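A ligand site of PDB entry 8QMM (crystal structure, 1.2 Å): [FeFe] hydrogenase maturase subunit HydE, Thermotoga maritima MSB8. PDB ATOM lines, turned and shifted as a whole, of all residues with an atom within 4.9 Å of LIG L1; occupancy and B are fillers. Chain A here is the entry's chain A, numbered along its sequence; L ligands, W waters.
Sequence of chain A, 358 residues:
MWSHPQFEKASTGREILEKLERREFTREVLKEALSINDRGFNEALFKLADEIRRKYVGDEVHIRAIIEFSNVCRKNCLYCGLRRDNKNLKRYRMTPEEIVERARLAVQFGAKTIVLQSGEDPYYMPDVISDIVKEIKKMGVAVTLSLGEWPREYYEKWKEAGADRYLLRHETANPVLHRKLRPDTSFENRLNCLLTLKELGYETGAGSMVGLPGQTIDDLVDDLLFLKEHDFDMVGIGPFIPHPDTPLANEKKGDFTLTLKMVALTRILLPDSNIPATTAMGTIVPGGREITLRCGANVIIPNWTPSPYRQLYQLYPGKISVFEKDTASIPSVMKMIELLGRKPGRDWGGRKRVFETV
An oxygen (O1) of LIG L1 is in salt-bridge range of the guanidinium group (NH2) of Arg 190. A nitrogen (N4) of LIG L1 sits at hydrogen-bond distance from the backbone carbonyl oxygen (O) of Tyr 79, 2.9 Å away. SG of Cys 80 binds FE1 of LG2 L2. The side-chain carboxylate (OE2) of Glu 171 lies within hydrogen-bond range of an oxygen (O4) of LIG L1, at 2.5 Å. The backbone NH (N) of Ile 241 is in hydrogen-bond range of a nitrogen (N5) of LIG L1 (3.0 Å). A nitrogen (N1) of LIG L1 lies close to the backbone carbonyl oxygen of Ser 118, 3.3 Å away. O of Ile 241 lies within hydrogen-bond range of N4 of LIG L1, at 2.8 Å. An oxygen (O5) of LIG L1 lies within hydrogen-bond range of the guanidinium group (NH2) of Arg 169.
O2 of LIG L1 is bound to FE4 of LG2 L2, 2.2 Å away.
NH2 of Arg 190 lies within salt-bridge range of OE2 of Glu 171, 3.2 Å away. OG of Ser 146 sits at hydrogen-bond distance from O of Leu 167, 3.4 Å away. The backbone carbonyl oxygen (O) of Ser 146 sits at hydrogen-bond distance from the backbone NH (N) of Ser 118, at 3.3 Å. The side-chain hydroxyl (OH) of Tyr 79 lies within hydrogen-bond range of the guanidinium group (NE) of Arg 182. The backbone carbonyl oxygen (O) of Glu 171 sits at hydrogen-bond distance from the backbone NH (N) of Met 209 (3.2 Å). The guanidinium group of Arg 190 lies within hydrogen-bond range of the backbone carbonyl oxygen of Arg 169 (2.7 Å). OH of Tyr 316 is in hydrogen-bond range of N of Ala 280 (3.1 Å). The side-chain hydroxyl of Tyr 313 lies within hydrogen-bond range of the side-chain amide oxygen of Gln 117 (2.9 Å).
N6 of LIG L1 lies close to SD of Met 209 (3.6 Å). CA of Cys 80 touches N3 of LIG L1, at 3.7 Å. Gln 117 touches LIG L1 (CD to C3, 3.7 Å). Ser 146 touches LIG L1. Gly 148 touches LIG L1. Pro 239 touches LIG L1. Phe 240 touches LIG L1. Tyr 313 touches LIG L1 (OH to C3, 3.4 Å). Leu 315 touches LIG L1. Tyr 316 touches LIG L1. Hydrophobic or aromatic side chains within 4 Å of LIG L1: Tyr 79, Met 209, Phe 240, Ile 241, Leu 315 and Tyr 316. The nearest printed residue that does not touch LIG L1 is Leu 168 (4.1 Å).
Water W1 bridges O1 of LIG L1 (2.8 Å) and N of Arg 169 (3.0 Å). Water W6 lies within hydrogen-bond range of O of Leu 167 (2.7 Å), O1 of LIG L1 (2.8 Å), OG of Ser 146 (3.0 Å), N of Gly 148 (3.0 Å) and N of Leu 147 (3.2 Å). Water W5 lies within hydrogen-bond range of N6 of LIG L1 and NH2 of Arg 169. Water W3 lies within hydrogen-bond range of the side-chain carboxylate of Glu 120, the guanidinium group of Arg 190, a sulfur (S1) of LG2 L2 and the guanidinium group of Arg 182. Water W2 lies within hydrogen-bond range of OH of Tyr 79, OE2 of Glu 171, NE of Arg 182 and S2 of LG2 L2.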
ATOM      1  N   TYR A  79       9.518  19.068  13.727  1.00  0.00           N
ATOM      2  CA  TYR A  79       9.912  17.838  14.426  1.00  0.00           C
ATOM      3  C   TYR A  79       8.740  16.995  14.909  1.00  0.00           C
ATOM      4  O   TYR A  79       8.934  15.833  15.260  1.00  0.00           O
ATOM      5  CB  TYR A  79      10.839  18.188  15.607  1.00  0.00           C
ATOM      6  CG  TYR A  79      10.336  19.327  16.447  1.00  0.00           C
ATOM      7  CD1 TYR A  79       9.360  19.138  17.389  1.00  0.00           C
ATOM      8  CD2 TYR A  79      10.851  20.579  16.279  1.00  0.00           C
ATOM      9  CE1 TYR A  79       8.889  20.200  18.163  1.00  0.00           C
ATOM     10  CE2 TYR A  79      10.412  21.638  17.043  1.00  0.00           C
ATOM     11  CZ  TYR A  79       9.418  21.443  17.970  1.00  0.00           C
ATOM     12  OH  TYR A  79       9.018  22.536  18.720  1.00  0.00           O
ATOM     13  N   CYS A  80       7.550  17.575  14.998  1.00  0.00           N
ATOM     14  CA  CYS A  80       6.485  16.994  15.809  1.00  0.00           C
ATOM     15  C   CYS A  80       5.447  16.251  14.980  1.00  0.00           C
ATOM     16  O   CYS A  80       4.912  16.778  13.990  1.00  0.00           O
ATOM     17  CB  CYS A  80       5.788  18.131  16.578  1.00  0.00           C
ATOM     18  SG  CYS A  80       4.479  17.554  17.681  1.00  0.00           S
ATOM     19  N   GLN A 117      -1.887  18.239  28.950  1.00  0.00           N
ATOM     20  CA  GLN A 117      -1.093  18.627  27.787  1.00  0.00           C
ATOM     21  C   GLN A 117      -1.910  18.385  26.543  1.00  0.00           C
ATOM     22  O   GLN A 117      -2.699  17.432  26.442  1.00  0.00           O
ATOM     23  CB  GLN A 117       0.213  17.813  27.709  1.00  0.00           C
ATOM     24  CG  GLN A 117       1.128  18.274  26.589  1.00  0.00           C
ATOM     25  CD  GLN A 117       2.430  17.552  26.575  1.00  0.00           C
ATOM     26  OE1 GLN A 117       2.516  16.464  26.025  1.00  0.00           O
ATOM     27  NE2 GLN A 117       3.435  18.099  27.191  1.00  0.00           N
ATOM     28  N   SER A 118      -1.687  19.213  25.529  1.00  0.00           N
ATOM     29  CA  SER A 118      -2.355  19.056  24.258  1.00  0.00           C
ATOM     30  C   SER A 118      -1.525  19.696  23.159  1.00  0.00           C
ATOM     31  O   SER A 118      -0.632  20.500  23.421  1.00  0.00           O
ATOM     32  CB  SER A 118      -3.724  19.667  24.304  1.00  0.00           C
ATOM     33  OG  SER A 118      -3.708  21.068  24.554  1.00  0.00           O
ATOM     34  N   GLY A 119      -1.915  19.393  21.919  1.00  0.00           N
ATOM     35  CA  GLY A 119      -1.601  20.317  20.835  1.00  0.00           C
ATOM     36  C   GLY A 119      -2.217  21.659  21.098  1.00  0.00           C
ATOM     37  O   GLY A 119      -3.071  21.817  21.989  1.00  0.00           O
ATOM     38  N   GLU A 120      -1.802  22.661  20.333  1.00  0.00           N
ATOM     39  CA  GLU A 120      -2.440  23.969  20.446  1.00  0.00           C
ATOM     40  C   GLU A 120      -3.790  23.884  19.742  1.00  0.00           C
ATOM     41  O   GLU A 120      -3.914  24.188  18.548  1.00  0.00           O
ATOM     42  CB  GLU A 120      -1.567  25.094  19.849  1.00  0.00           C
ATOM     43  CG  GLU A 120      -0.297  25.333  20.629  1.00  0.00           C
ATOM     44  CD  GLU A 120       0.390  26.611  20.255  1.00  0.00           C
ATOM     45  OE1 GLU A 120      -0.172  27.372  19.448  1.00  0.00           O
ATOM     46  OE2 GLU A 120       1.505  26.845  20.789  1.00  0.00           O
ATOM     47  N   SER A 146       0.296  22.343  29.969  1.00  0.00           N
ATOM     48  CA  SER A 146       1.297  22.328  28.923  1.00  0.00           C
ATOM     49  C   SER A 146       0.535  22.436  27.602  1.00  0.00           C
ATOM     50  O   SER A 146       0.328  21.436  26.904  1.00  0.00           O
ATOM     51  CB  SER A 146       2.131  21.064  29.032  1.00  0.00           C
ATOM     52  OG  SER A 146       3.176  21.005  28.069  1.00  0.00           O
ATOM     53  N   LEU A 147       0.093  23.637  27.272  1.00  0.00           N
ATOM     54  CA  LEU A 147      -0.831  23.851  26.164  1.00  0.00           C
ATOM     55  C   LEU A 147      -0.236  24.699  25.054  1.00  0.00           C
ATOM     56  O   LEU A 147      -0.930  25.006  24.095  1.00  0.00           O
ATOM     57  CB  LEU A 147      -2.121  24.521  26.662  1.00  0.00           C
ATOM     58  CG  LEU A 147      -2.719  23.899  27.930  1.00  0.00           C
ATOM     59  CD1 LEU A 147      -3.980  24.624  28.313  1.00  0.00           C
ATOM     60  CD2 LEU A 147      -3.047  22.416  27.730  1.00  0.00           C
ATOM     61  N   GLY A 148       1.028  25.069  25.155  1.00  0.00           N
ATOM     62  CA  GLY A 148       1.655  25.895  24.126  1.00  0.00           C
ATOM     63  C   GLY A 148       1.544  27.378  24.382  1.00  0.00           C
ATOM     64  O   GLY A 148       1.399  27.826  25.526  1.00  0.00           O
ATOM     65  N   LEU A 167       4.322  24.172  31.745  1.00  0.00           N
ATOM     66  CA  LEU A 167       5.474  23.650  31.029  1.00  0.00           C
ATOM     67  C   LEU A 167       5.487  24.201  29.617  1.00  0.00           C
ATOM     68  O   LEU A 167       4.511  24.009  28.881  1.00  0.00           O
ATOM     69  CB  LEU A 167       5.429  22.141  30.937  1.00  0.00           C
ATOM     70  CG  LEU A 167       5.188  21.413  32.239  1.00  0.00           C
ATOM     71  CD1 LEU A 167       5.119  19.919  31.986  1.00  0.00           C
ATOM     72  CD2 LEU A 167       6.211  21.764  33.272  1.00  0.00           C
ATOM     73  N   LEU A 168       6.550  24.875  29.235  1.00  0.00           N
ATOM     74  CA  LEU A 168       6.695  25.429  27.901  1.00  0.00           C
ATOM     75  C   LEU A 168       8.158  25.295  27.509  1.00  0.00           C
ATOM     76  O   LEU A 168       8.928  26.220  27.717  1.00  0.00           O
ATOM     77  CB  LEU A 168       6.186  26.856  27.858  1.00  0.00           C
ATOM     78  CG  LEU A 168       6.009  27.399  26.439  1.00  0.00           C
ATOM     79  CD1 LEU A 168       4.800  26.813  25.780  1.00  0.00           C
ATOM     80  CD2 LEU A 168       5.856  28.911  26.496  1.00  0.00           C
ATOM     81  N   ARG A 169       8.537  24.121  27.007  1.00  0.00           N
ATOM     82  CA  ARG A 169       9.947  23.932  26.673  1.00  0.00           C
ATOM     83  C   ARG A 169      10.371  24.998  25.696  1.00  0.00           C
ATOM     84  O   ARG A 169       9.632  25.330  24.766  1.00  0.00           O
ATOM     85  CB  ARG A 169      10.149  22.575  26.063  1.00  0.00           C
ATOM     86  CG  ARG A 169       9.949  21.449  27.063  1.00  0.00           C
ATOM     87  CD  ARG A 169      10.363  20.171  26.384  1.00  0.00           C
ATOM     88  NE  ARG A 169      10.021  19.068  27.197  1.00  0.00           N
ATOM     89  CZ  ARG A 169      10.308  17.834  26.826  1.00  0.00           C
ATOM     90  NH1 ARG A 169      10.163  16.854  27.688  1.00  0.00           N
ATOM     91  NH2 ARG A 169      10.786  17.617  25.626  1.00  0.00           N
ATOM     92  N   GLU A 171      12.722  24.644  23.580  1.00  0.00           N
ATOM     93  CA  GLU A 171      13.025  23.824  22.420  1.00  0.00           C
ATOM     94  C   GLU A 171      14.456  23.972  21.956  1.00  0.00           C
ATOM     95  O   GLU A 171      15.189  22.991  21.879  1.00  0.00           O
ATOM     96  CB  GLU A 171      12.045  24.038  21.274  1.00  0.00           C
ATOM     97  CG  GLU A 171      10.563  24.001  21.675  1.00  0.00           C
ATOM     98  CD  GLU A 171      10.061  22.722  22.295  1.00  0.00           C
ATOM     99  OE1 GLU A 171      10.817  21.773  22.543  1.00  0.00           O
ATOM    100  OE2 GLU A 171       8.847  22.684  22.549  1.00  0.00           O
ATOM    101  N   ARG A 182      10.175  25.915  13.842  1.00  0.00           N
ATOM    102  CA  ARG A 182       8.878  26.291  14.403  1.00  0.00           C
ATOM    103  C   ARG A 182       8.387  27.479  13.600  1.00  0.00           C
ATOM    104  O   ARG A 182       8.408  28.620  14.061  1.00  0.00           O
ATOM    105  CB  ARG A 182       9.000  26.573  15.888  1.00  0.00           C
ATOM    106  CG  ARG A 182       9.715  25.438  16.633  1.00  0.00           C
ATOM    107  CD  ARG A 182       9.592  25.575  18.155  1.00  0.00           C
ATOM    108  NE  ARG A 182       8.226  25.386  18.605  1.00  0.00           N
ATOM    109  CZ  ARG A 182       7.440  26.340  19.095  1.00  0.00           C
ATOM    110  NH1 ARG A 182       7.901  27.525  19.477  1.00  0.00           N
ATOM    111  NH2 ARG A 182       6.129  26.068  19.279  1.00  0.00           N
ATOM    112  N   ARG A 190       8.335  32.595  22.344  1.00  0.00           N
ATOM    113  CA  ARG A 190       8.417  31.517  23.310  1.00  0.00           C
ATOM    114  C   ARG A 190       8.888  32.080  24.654  1.00  0.00           C
ATOM    115  O   ARG A 190       8.341  31.767  25.715  1.00  0.00           O
ATOM    116  CB  ARG A 190       9.369  30.388  22.784  1.00  0.00           C
ATOM    117  CG  ARG A 190       9.206  29.063  23.475  1.00  0.00           C
ATOM    118  CD  ARG A 190       8.004  28.383  23.004  1.00  0.00           C
ATOM    119  NE  ARG A 190       7.972  26.960  23.384  1.00  0.00           N
ATOM    120  CZ  ARG A 190       6.933  26.161  23.169  1.00  0.00           C
ATOM    121  NH1 ARG A 190       5.903  26.610  22.514  1.00  0.00           N
ATOM    122  NH2 ARG A 190       6.945  24.934  23.664  1.00  0.00           N
ATOM    123  N   MET A 209      15.161  20.079  23.283  1.00  0.00           N
ATOM    124  CA  MET A 209      15.478  18.806  22.665  1.00  0.00           C
ATOM    125  C   MET A 209      16.938  18.791  22.327  1.00  0.00           C
ATOM    126  O   MET A 209      17.569  19.840  22.053  1.00  0.00           O
ATOM    127  CB  MET A 209      14.640  18.599  21.414  1.00  0.00           C
ATOM    128  CG  MET A 209      13.215  18.215  21.692  1.00  0.00           C
ATOM    129  SD  MET A 209      12.188  18.179  20.207  1.00  0.00           S
ATOM    130  CE  MET A 209      12.027  19.911  19.923  1.00  0.00           C
ATOM    131  N   PRO A 239      15.895  13.679  24.009  1.00  0.00           N
ATOM    132  CA  PRO A 239      16.456  13.619  22.678  1.00  0.00           C
ATOM    133  C   PRO A 239      15.390  13.898  21.633  1.00  0.00           C
ATOM    134  O   PRO A 239      14.219  13.535  21.786  1.00  0.00           O
ATOM    135  CB  PRO A 239      16.894  12.159  22.556  1.00  0.00           C
ATOM    136  CG  PRO A 239      15.876  11.403  23.423  1.00  0.00           C
ATOM    137  CD  PRO A 239      15.603  12.390  24.563  1.00  0.00           C
ATOM    138  N   PHE A 240      15.805  14.551  20.541  1.00  0.00           N
ATOM    139  CA  PHE A 240      14.981  14.616  19.350  1.00  0.00           C
ATOM    140  C   PHE A 240      14.821  13.210  18.756  1.00  0.00           C
ATOM    141  O   PHE A 240      15.823  12.522  18.515  1.00  0.00           O
ATOM    142  CB  PHE A 240      15.641  15.526  18.341  1.00  0.00           C
ATOM    143  CG  PHE A 240      15.086  15.385  16.942  1.00  0.00           C
ATOM    144  CD1 PHE A 240      13.757  15.637  16.671  1.00  0.00           C
ATOM    145  CD2 PHE A 240      15.901  14.973  15.920  1.00  0.00           C
ATOM    146  CE1 PHE A 240      13.251  15.468  15.396  1.00  0.00           C
ATOM    147  CE2 PHE A 240      15.395  14.804  14.645  1.00  0.00           C
ATOM    148  CZ  PHE A 240      14.052  15.052  14.404  1.00  0.00           C
ATOM    149  N   ILE A 241      13.598  12.783  18.500  1.00  0.00           N
ATOM    150  CA  ILE A 241      13.328  11.504  17.912  1.00  0.00           C
ATOM    151  C   ILE A 241      12.607  11.723  16.602  1.00  0.00           C
ATOM    152  O   ILE A 241      11.457  12.190  16.586  1.00  0.00           O
ATOM    153  CB  ILE A 241      12.502  10.612  18.863  1.00  0.00           C
ATOM    154  CG1 ILE A 241      13.272  10.413  20.165  1.00  0.00           C
ATOM    155  CG2 ILE A 241      12.180   9.300  18.212  1.00  0.00           C
ATOM    156  CD1 ILE A 241      12.521   9.693  21.244  1.00  0.00           C
ATOM    157  N   PRO A 242      13.224  11.454  15.454  1.00  0.00           N
ATOM    158  CA  PRO A 242      12.593  11.767  14.181  1.00  0.00           C
ATOM    159  C   PRO A 242      11.293  11.015  14.013  1.00  0.00           C
ATOM    160  O   PRO A 242      11.184   9.808  14.309  1.00  0.00           O
ATOM    161  CB  PRO A 242      13.647  11.280  13.143  1.00  0.00           C
ATOM    162  CG  PRO A 242      14.960  11.274  13.868  1.00  0.00           C
ATOM    163  CD  PRO A 242      14.630  11.004  15.330  1.00  0.00           C
ATOM    164  N   ALA A 280      10.853  10.492  26.364  1.00  0.00           N
ATOM    165  CA  ALA A 280      11.752  10.363  25.225  1.00  0.00           C
ATOM    166  C   ALA A 280      13.025   9.622  25.587  1.00  0.00           C
ATOM    167  O   ALA A 280      13.557   8.816  24.825  1.00  0.00           O
ATOM    168  CB  ALA A 280      12.009  11.696  24.590  1.00  0.00           C
ATOM    169  N   TYR A 313      -1.412  10.070  20.332  1.00  0.00           N
ATOM    170  CA  TYR A 313      -0.641  11.245  20.744  1.00  0.00           C
ATOM    171  C   TYR A 313       0.816  11.013  20.372  1.00  0.00           C
ATOM    172  O   TYR A 313       1.704  10.888  21.198  1.00  0.00           O
ATOM    173  CB  TYR A 313      -0.843  11.559  22.220  1.00  0.00           C
ATOM    174  CG  TYR A 313      -0.414  12.951  22.574  1.00  0.00           C
ATOM    175  CD1 TYR A 313      -1.214  14.060  22.351  1.00  0.00           C
ATOM    176  CD2 TYR A 313       0.805  13.159  23.192  1.00  0.00           C
ATOM    177  CE1 TYR A 313      -0.861  15.332  22.732  1.00  0.00           C
ATOM    178  CE2 TYR A 313       1.196  14.421  23.604  1.00  0.00           C
ATOM    179  CZ  TYR A 313       0.371  15.491  23.362  1.00  0.00           C
ATOM    180  OH  TYR A 313       0.754  16.730  23.775  1.00  0.00           O
ATOM    181  N   LEU A 315       3.806  12.129  19.225  1.00  0.00           N
ATOM    182  CA  LEU A 315       4.798  13.197  19.053  1.00  0.00           C
ATOM    183  C   LEU A 315       5.979  12.622  18.292  1.00  0.00           C
ATOM    184  O   LEU A 315       6.551  13.311  17.405  1.00  0.00           O
ATOM    185  CB  LEU A 315       5.324  13.701  20.395  1.00  0.00           C
ATOM    186  CG  LEU A 315       4.312  14.282  21.359  1.00  0.00           C
ATOM    187  CD1 LEU A 315       5.017  14.565  22.679  1.00  0.00           C
ATOM    188  CD2 LEU A 315       3.674  15.561  20.829  1.00  0.00           C
ATOM    189  N   TYR A 316       6.385  11.391  18.605  1.00  0.00           N
ATOM    190  CA  TYR A 316       7.516  10.703  18.009  1.00  0.00           C
ATOM    191  C   TYR A 316       7.220   9.214  18.073  1.00  0.00           C
ATOM    192  O   TYR A 316       6.472   8.764  18.946  1.00  0.00           O
ATOM    193  CB  TYR A 316       8.833  11.073  18.732  1.00  0.00           C
ATOM    194  CG  TYR A 316       8.747  11.005  20.228  1.00  0.00           C
ATOM    195  CD1 TYR A 316       8.911   9.791  20.906  1.00  0.00           C
ATOM    196  CD2 TYR A 316       8.538  12.124  20.971  1.00  0.00           C
ATOM    197  CE1 TYR A 316       8.853   9.761  22.301  1.00  0.00           C
ATOM    198  CE2 TYR A 316       8.471  12.111  22.350  1.00  0.00           C
ATOM    199  CZ  TYR A 316       8.579  10.887  22.986  1.00  0.00           C
ATOM    200  OH  TYR A 316       8.537  10.782  24.380  1.00  0.00           O
HETATM  201  N1  LIG L   1       2.017  21.874  22.080  1.00  0.00           N
HETATM  202  C1  LIG L   1       2.670  22.071  23.379  1.00  0.00           C
HETATM  203  C2  LIG L   1       2.622  20.781  24.193  1.00  0.00           C
HETATM  204  C3  LIG L   1       2.755  19.456  23.449  1.00  0.00           C
HETATM  205  S1  LIG L   1       4.294  19.159  22.557  1.00  0.00           S
HETATM  206  C4  LIG L   1       4.078  22.604  23.157  1.00  0.00           C
HETATM  207  O1  LIG L   1       4.685  23.099  24.126  1.00  0.00           O
HETATM  208  O2  LIG L   1       4.534  22.503  21.986  1.00  0.00           O
HETATM  209  C5  LIG L   1       5.331  18.700  23.991  1.00  0.00           C
HETATM  210  C6  LIG L   1       6.840  18.579  23.729  1.00  0.00           C
HETATM  211  O3  LIG L   1       7.085  17.390  22.979  1.00  0.00           O
HETATM  212  C7  LIG L   1       7.529  19.620  22.925  1.00  0.00           C
HETATM  213  O4  LIG L   1       7.876  20.690  23.776  1.00  0.00           O
HETATM  214  C8  LIG L   1       8.776  18.923  22.378  1.00  0.00           C
HETATM  215  O5  LIG L   1       9.946  19.213  23.119  1.00  0.00           O
HETATM  216  C9  LIG L   1       8.403  17.441  22.506  1.00  0.00           C
HETATM  217  N2  LIG L   1       8.538  16.780  21.218  1.00  0.00           N
HETATM  218  C10 LIG L   1       7.804  17.038  20.089  1.00  0.00           C
HETATM  219  N3  LIG L   1       8.246  16.354  19.057  1.00  0.00           N
HETATM  220  C11 LIG L   1       9.348  15.649  19.489  1.00  0.00           C
HETATM  221  C12 LIG L   1      10.223  14.763  18.871  1.00  0.00           C
HETATM  222  N4  LIG L   1      10.112  14.467  17.567  1.00  0.00           N
HETATM  223  N5  LIG L   1      11.238  14.240  19.612  1.00  0.00           N
HETATM  224  C13 LIG L   1      11.308  14.543  20.915  1.00  0.00           C
HETATM  225  N6  LIG L   1      10.494  15.345  21.588  1.00  0.00           N
HETATM  226  C14 LIG L   1       9.516  15.920  20.840  1.00  0.00           C
HETATM  227 FE1  LG2 L   2       3.745  19.610  18.286  1.00  0.00          FE
HETATM  228 FE2  LG2 L   2       1.889  21.542  18.065  1.00  0.00          FE
HETATM  229 FE3  LG2 L   2       4.509  22.165  17.866  1.00  0.00          FE
HETATM  230 FE4  LG2 L   2       3.453  21.460  20.441  1.00  0.00          FE
HETATM  231  S1  LG2 L   2       2.978  23.321  19.056  1.00  0.00           S
HETATM  232  S2  LG2 L   2       5.421  20.711  19.417  1.00  0.00           S
HETATM  233  S3  LG2 L   2       1.925  19.846  19.582  1.00  0.00           S
HETATM  234  S4  LG2 L   2       3.295  20.884  16.400  1.00  0.00           S
HETATM  235  O   HOH W   1       6.641  22.165  25.852  1.00  0.00           O
HETATM  236  O   HOH W   2       7.132  23.235  20.511  1.00  0.00           O
HETATM  237  O   HOH W   3       3.632  25.361  21.480  1.00  0.00           O
HETATM  238  O   HOH W   4       7.285  15.756  25.452  1.00  0.00           O
HETATM  239  O   HOH W   5      11.914  15.319  24.144  1.00  0.00           O
HETATM  240  O   HOH W   6       3.254  23.539  26.538  1.00  0.00           O
